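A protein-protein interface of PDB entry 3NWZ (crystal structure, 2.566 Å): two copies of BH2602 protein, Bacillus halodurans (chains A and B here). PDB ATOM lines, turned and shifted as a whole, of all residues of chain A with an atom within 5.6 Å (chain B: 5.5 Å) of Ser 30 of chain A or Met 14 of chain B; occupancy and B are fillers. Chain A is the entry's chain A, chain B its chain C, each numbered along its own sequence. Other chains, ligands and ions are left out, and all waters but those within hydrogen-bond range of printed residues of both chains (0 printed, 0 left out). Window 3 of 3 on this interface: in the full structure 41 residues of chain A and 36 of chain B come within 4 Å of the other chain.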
ATOM      1  N   GLU A  25      29.772 -29.482  -7.587  1.00  0.00           N
ATOM      2  CA  GLU A  25      28.770 -28.434  -7.769  1.00  0.00           C
ATOM      3  C   GLU A  25      29.365 -27.198  -8.455  1.00  0.00           C
ATOM      4  O   GLU A  25      28.761 -26.638  -9.370  1.00  0.00           O
ATOM      5  CB  GLU A  25      28.179 -28.013  -6.422  1.00  0.00           C
ATOM      6  CG  GLU A  25      27.599 -29.133  -5.546  1.00  0.00           C
ATOM      7  CD  GLU A  25      27.048 -28.602  -4.215  1.00  0.00           C
ATOM      8  OE1 GLU A  25      27.750 -27.824  -3.533  1.00  0.00           O
ATOM      9  OE2 GLU A  25      25.914 -28.964  -3.842  1.00  0.00           O
ATOM     10  N   LYS A  26      30.538 -26.757  -8.013  1.00  0.00           N
ATOM     11  CA  LYS A  26      31.151 -25.589  -8.639  1.00  0.00           C
ATOM     12  C   LYS A  26      31.609 -25.971 -10.037  1.00  0.00           C
ATOM     13  O   LYS A  26      31.614 -25.153 -10.956  1.00  0.00           O
ATOM     14  CB  LYS A  26      32.346 -25.086  -7.825  1.00  0.00           C
ATOM     15  CG  LYS A  26      31.988 -24.257  -6.599  1.00  0.00           C
ATOM     16  CD  LYS A  26      33.257 -23.842  -5.870  1.00  0.00           C
ATOM     17  CE  LYS A  26      32.981 -22.923  -4.693  1.00  0.00           C
ATOM     18  NZ  LYS A  26      34.248 -22.450  -4.058  1.00  0.00           N
ATOM     19  N   ASP A  27      31.993 -27.229 -10.194  1.00  0.00           N
ATOM     20  CA  ASP A  27      32.445 -27.719 -11.491  1.00  0.00           C
ATOM     21  C   ASP A  27      31.269 -27.754 -12.468  1.00  0.00           C
ATOM     22  O   ASP A  27      31.411 -27.426 -13.648  1.00  0.00           O
ATOM     23  CB  ASP A  27      33.010 -29.129 -11.346  1.00  0.00           C
ATOM     24  CG  ASP A  27      33.937 -29.489 -12.466  1.00  0.00           C
ATOM     25  OD1 ASP A  27      35.158 -29.275 -12.300  1.00  0.00           O
ATOM     26  OD2 ASP A  27      33.441 -29.968 -13.510  1.00  0.00           O
ATOM     27  N   VAL A  28      30.108 -28.165 -11.969  1.00  0.00           N
ATOM     28  CA  VAL A  28      28.929 -28.235 -12.805  1.00  0.00           C
ATOM     29  C   VAL A  28      28.602 -26.877 -13.395  1.00  0.00           C
ATOM     30  O   VAL A  28      28.716 -26.691 -14.617  1.00  0.00           O
ATOM     31  CB  VAL A  28      27.694 -28.733 -12.028  1.00  0.00           C
ATOM     32  CG1 VAL A  28      26.433 -28.578 -12.898  1.00  0.00           C
ATOM     33  CG2 VAL A  28      27.880 -30.181 -11.634  1.00  0.00           C
ATOM     34  N   LEU A  29      28.202 -25.937 -12.530  1.00  0.00           N
ATOM     35  CA  LEU A  29      27.826 -24.587 -12.956  1.00  0.00           C
ATOM     36  C   LEU A  29      28.774 -23.993 -13.982  1.00  0.00           C
ATOM     37  O   LEU A  29      28.354 -23.324 -14.926  1.00  0.00           O
ATOM     38  CB  LEU A  29      27.758 -23.660 -11.763  1.00  0.00           C
ATOM     39  CG  LEU A  29      27.315 -22.231 -12.085  1.00  0.00           C
ATOM     40  CD1 LEU A  29      26.020 -22.290 -12.858  1.00  0.00           C
ATOM     41  CD2 LEU A  29      27.131 -21.428 -10.802  1.00  0.00           C
ATOM     42  N   SER A  30      30.059 -24.242 -13.788  1.00  0.00           N
ATOM     43  CA  SER A  30      31.075 -23.749 -14.702  1.00  0.00           C
ATOM     44  C   SER A  30      30.718 -24.198 -16.125  1.00  0.00           C
ATOM     45  O   SER A  30      30.685 -23.384 -17.059  1.00  0.00           O
ATOM     46  CB  SER A  30      32.437 -24.308 -14.285  1.00  0.00           C
ATOM     47  OG  SER A  30      33.487 -23.681 -14.984  1.00  0.00           O
ATOM     48  N   SER A  31      30.434 -25.491 -16.283  1.00  0.00           N
ATOM     49  CA  SER A  31      30.077 -26.024 -17.585  1.00  0.00           C
ATOM     50  C   SER A  31      28.797 -25.364 -18.016  1.00  0.00           C
ATOM     51  O   SER A  31      28.708 -24.799 -19.108  1.00  0.00           O
ATOM     52  CB  SER A  31      29.878 -27.538 -17.522  1.00  0.00           C
ATOM     53  OG  SER A  31      31.114 -28.223 -17.616  1.00  0.00           O
ATOM     54  N   ILE A  32      27.799 -25.434 -17.142  1.00  0.00           N
ATOM     55  CA  ILE A  32      26.510 -24.831 -17.435  1.00  0.00           C
ATOM     56  C   ILE A  32      26.686 -23.417 -17.952  1.00  0.00           C
ATOM     57  O   ILE A  32      26.156 -23.084 -19.007  1.00  0.00           O
ATOM     58  CB  ILE A  32      25.593 -24.821 -16.194  1.00  0.00           C
ATOM     59  CG1 ILE A  32      25.091 -26.242 -15.931  1.00  0.00           C
ATOM     60  CG2 ILE A  32      24.429 -23.866 -16.407  1.00  0.00           C
ATOM     61  CD1 ILE A  32      24.087 -26.350 -14.813  1.00  0.00           C
ATOM     62  N   VAL A  33      27.432 -22.578 -17.237  1.00  0.00           N
ATOM     63  CA  VAL A  33      27.607 -21.215 -17.724  1.00  0.00           C
ATOM     64  C   VAL A  33      28.195 -21.241 -19.146  1.00  0.00           C
ATOM     65  O   VAL A  33      27.718 -20.521 -20.025  1.00  0.00           O
ATOM     66  CB  VAL A  33      28.515 -20.360 -16.788  1.00  0.00           C
ATOM     67  CG1 VAL A  33      28.348 -18.871 -17.129  1.00  0.00           C
ATOM     68  CG2 VAL A  33      28.156 -20.600 -15.329  1.00  0.00           C
ATOM     69  N   ASP A  34      29.217 -22.069 -19.379  1.00  0.00           N
ATOM     70  CA  ASP A  34      29.810 -22.174 -20.717  1.00  0.00           C
ATOM     71  C   ASP A  34      28.712 -22.512 -21.726  1.00  0.00           C
ATOM     72  O   ASP A  34      28.631 -21.925 -22.804  1.00  0.00           O
ATOM     73  CB  ASP A  34      30.858 -23.295 -20.786  1.00  0.00           C
ATOM     74  CG  ASP A  34      32.117 -22.984 -20.009  1.00  0.00           C
ATOM     75  OD1 ASP A  34      32.610 -21.840 -20.092  1.00  0.00           O
ATOM     76  OD2 ASP A  34      32.623 -23.903 -19.335  1.00  0.00           O
ATOM     77  N   GLY A  35      27.882 -23.486 -21.362  1.00  0.00           N
ATOM     78  CA  GLY A  35      26.799 -23.908 -22.227  1.00  0.00           C
ATOM     79  C   GLY A  35      25.997 -22.714 -22.667  1.00  0.00           C
ATOM     80  O   GLY A  35      26.069 -22.319 -23.834  1.00  0.00           O
ATOM     81  N   LEU A  37      26.418 -19.786 -22.494  1.00  0.00           N
ATOM     82  CA  LEU A  37      27.263 -18.814 -23.164  1.00  0.00           C
ATOM     83  C   LEU A  37      27.446 -19.193 -24.628  1.00  0.00           C
ATOM     84  O   LEU A  37      27.414 -18.335 -25.508  1.00  0.00           O
ATOM     85  CB  LEU A  37      28.619 -18.752 -22.446  1.00  0.00           C
ATOM     86  CG  LEU A  37      29.299 -17.395 -22.257  1.00  0.00           C
ATOM     87  CD1 LEU A  37      28.266 -16.325 -22.003  1.00  0.00           C
ATOM     88  CD2 LEU A  37      30.282 -17.480 -21.099  1.00  0.00           C
ATOM     89  N   ILE B  10      36.228 -19.117 -11.509  1.00  0.00           N
ATOM     90  CA  ILE B  10      36.091 -17.823 -12.246  1.00  0.00           C
ATOM     91  C   ILE B  10      34.736 -17.753 -12.951  1.00  0.00           C
ATOM     92  O   ILE B  10      34.525 -16.905 -13.824  1.00  0.00           O
ATOM     93  CB  ILE B  10      37.212 -17.659 -13.313  1.00  0.00           C
ATOM     94  CG1 ILE B  10      36.882 -18.464 -14.580  1.00  0.00           C
ATOM     95  CG2 ILE B  10      38.543 -18.125 -12.737  1.00  0.00           C
ATOM     96  CD1 ILE B  10      36.701 -19.959 -14.359  1.00  0.00           C
ATOM     97  N   VAL B  11      33.825 -18.645 -12.564  1.00  0.00           N
ATOM     98  CA  VAL B  11      32.502 -18.695 -13.172  1.00  0.00           C
ATOM     99  C   VAL B  11      31.836 -17.314 -13.208  1.00  0.00           C
ATOM    100  O   VAL B  11      31.212 -16.947 -14.210  1.00  0.00           O
ATOM    101  CB  VAL B  11      31.567 -19.733 -12.449  1.00  0.00           C
ATOM    102  CG1 VAL B  11      32.401 -20.698 -11.577  1.00  0.00           C
ATOM    103  CG2 VAL B  11      30.491 -19.018 -11.637  1.00  0.00           C
ATOM    104  N   ASP B  12      31.975 -16.548 -12.127  1.00  0.00           N
ATOM    105  CA  ASP B  12      31.391 -15.211 -12.068  1.00  0.00           C
ATOM    106  C   ASP B  12      31.831 -14.331 -13.234  1.00  0.00           C
ATOM    107  O   ASP B  12      31.057 -13.515 -13.747  1.00  0.00           O
ATOM    108  CB  ASP B  12      31.755 -14.539 -10.752  1.00  0.00           C
ATOM    109  CG  ASP B  12      30.697 -14.733  -9.704  1.00  0.00           C
ATOM    110  OD1 ASP B  12      29.573 -14.222  -9.909  1.00  0.00           O
ATOM    111  OD2 ASP B  12      30.987 -15.401  -8.689  1.00  0.00           O
ATOM    112  N   LYS B  13      33.087 -14.496 -13.638  1.00  0.00           N
ATOM    113  CA  LYS B  13      33.626 -13.746 -14.761  1.00  0.00           C
ATOM    114  C   LYS B  13      32.779 -14.157 -15.973  1.00  0.00           C
ATOM    115  O   LYS B  13      32.283 -13.312 -16.727  1.00  0.00           O
ATOM    116  CB  LYS B  13      35.096 -14.123 -14.975  1.00  0.00           C
ATOM    117  CG  LYS B  13      35.991 -12.962 -15.379  1.00  0.00           C
ATOM    118  CD  LYS B  13      37.461 -13.361 -15.340  1.00  0.00           C
ATOM    119  CE  LYS B  13      38.366 -12.208 -15.765  1.00  0.00           C
ATOM    120  NZ  LYS B  13      38.240 -11.013 -14.881  1.00  0.00           N
ATOM    121  N   MET B  14      32.590 -15.465 -16.126  1.00  0.00           N
ATOM    122  CA  MET B  14      31.800 -15.994 -17.226  1.00  0.00           C
ATOM    123  C   MET B  14      30.321 -15.603 -17.128  1.00  0.00           C
ATOM    124  O   MET B  14      29.682 -15.357 -18.151  1.00  0.00           O
ATOM    125  CB  MET B  14      31.910 -17.519 -17.277  1.00  0.00           C
ATOM    126  CG  MET B  14      33.318 -18.049 -17.469  1.00  0.00           C
ATOM    127  SD  MET B  14      33.406 -19.981 -17.620  1.00  0.00           S
ATOM    128  CE  MET B  14      33.684 -20.430 -15.765  1.00  0.00           C
ATOM    129  N   GLU B  15      29.765 -15.548 -15.918  1.00  0.00           N
ATOM    130  CA  GLU B  15      28.355 -15.198 -15.806  1.00  0.00           C
ATOM    131  C   GLU B  15      28.006 -13.785 -16.257  1.00  0.00           C
ATOM    132  O   GLU B  15      27.034 -13.205 -15.780  1.00  0.00           O
ATOM    133  CB  GLU B  15      27.822 -15.455 -14.387  1.00  0.00           C
ATOM    134  CG  GLU B  15      27.279 -16.878 -14.204  1.00  0.00           C
ATOM    135  CD  GLU B  15      26.455 -17.071 -12.929  1.00  0.00           C
ATOM    136  OE1 GLU B  15      25.585 -16.216 -12.644  1.00  0.00           O
ATOM    137  OE2 GLU B  15      26.662 -18.089 -12.223  1.00  0.00           O
ATOM    138  N   ARG B  16      28.801 -13.236 -17.179  1.00  0.00           N
ATOM    139  CA  ARG B  16      28.545 -11.909 -17.745  1.00  0.00           C
ATOM    140  C   ARG B  16      27.750 -12.181 -19.022  1.00  0.00           C
ATOM    141  O   ARG B  16      27.565 -11.317 -19.881  1.00  0.00           O
ATOM    142  CB  ARG B  16      29.845 -11.184 -18.077  1.00  0.00           C
ATOM    143  CG  ARG B  16      30.237 -11.192 -19.549  1.00  0.00           C
ATOM    144  CD  ARG B  16      30.670 -12.560 -20.025  1.00  0.00           C
ATOM    145  NE  ARG B  16      31.418 -12.467 -21.272  1.00  0.00           N
ATOM    146  CZ  ARG B  16      32.188 -13.436 -21.756  1.00  0.00           C
ATOM    147  NH1 ARG B  16      32.312 -14.579 -21.098  1.00  0.00           N
ATOM    148  NH2 ARG B  16      32.849 -13.258 -22.892  1.00  0.00           N
ATOM    149  N   PHE B  17      27.308 -13.428 -19.125  1.00  0.00           N
ATOM    150  CA  PHE B  17      26.486 -13.924 -20.217  1.00  0.00           C
ATOM    151  C   PHE B  17      25.226 -13.044 -20.192  1.00  0.00           C
ATOM    152  O   PHE B  17      24.354 -13.123 -21.054  1.00  0.00           O
ATOM    153  CB  PHE B  17      26.212 -15.415 -19.909  1.00  0.00           C
ATOM    154  CG  PHE B  17      24.789 -15.870 -20.113  1.00  0.00           C
ATOM    155  CD1 PHE B  17      24.399 -16.460 -21.310  1.00  0.00           C
ATOM    156  CD2 PHE B  17      23.863 -15.777 -19.080  1.00  0.00           C
ATOM    157  CE1 PHE B  17      23.104 -16.959 -21.475  1.00  0.00           C
ATOM    158  CE2 PHE B  17      22.566 -16.274 -19.239  1.00  0.00           C
ATOM    159  CZ  PHE B  17      22.189 -16.869 -20.443  1.00  0.00           C
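The side-chain carboxylate (OD1) of Asp 34 of chain A sits close to the side-chain sulfur (SD) of Met 14 of chain B, at 3.2 Å.
Among the printed residues, pairs that only touch across the chains: Leu 29 of chain A with Glu 15 of chain B (3.7 Å), Ser 30 of chain A with Met 14 of chain B (3.3 Å), Val 33 of chain A with Met 14 of chain B (3.8 Å), Val 33 of chain A with Glu 15 of chain B (3.7 Å), Leu 37 of chain A with Met 14 of chain B (3.7 Å), Leu 37 of chain A with Arg 16 of chain B (3.5 Å) and Leu 37 of chain A with Phe 17 of chain B (3.1 Å).
Glu 25 of chain A touches none of the printed residues of chain B.
Of the printed residues of chain B, Leu 29 of chain A touches Glu 15 (3.7 Å).
Of the printed residues of chain B, Ser 30 of chain A touches Met 14.
Of the printed residues of chain B, Leu 37 of chain A touches Met 14 (3.7 Å), Arg 16 (3.5 Å) and Phe 17 (3.1 Å).
Val 11 of chain B touches none of the printed residues of chain A.
Of chain A, only Ser 30, Val 33, Asp 34 and Leu 37 come within 4 Å of Met 14 of chain B.
Printed residues of chain A within 4 Å of Glu 15 of chain B: Leu 29 (3.7 Å) and Val 33 (3.7 Å).
The nearest printed residue of chain A that does not touch Met 14 of chain B is Ser 31 of chain A (6.0 Å).
Hydrophobic or aromatic side chains of chain A within 4 Å of the printed part of chain B: Leu 29, Val 33 and Leu 37.
Of the 8 printed residues of chain B, 4 touch a printed residue of chain A.
Hydrophobic or aromatic side chains of chain B within 4 Å of the printed part of chain A: Met 14 and Phe 17.
Among the printed residues, no Asp or Glu carboxylate lies within 4 Å of a Lys or Arg side-chain nitrogen of the other chain.
No position is printed for both chains.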
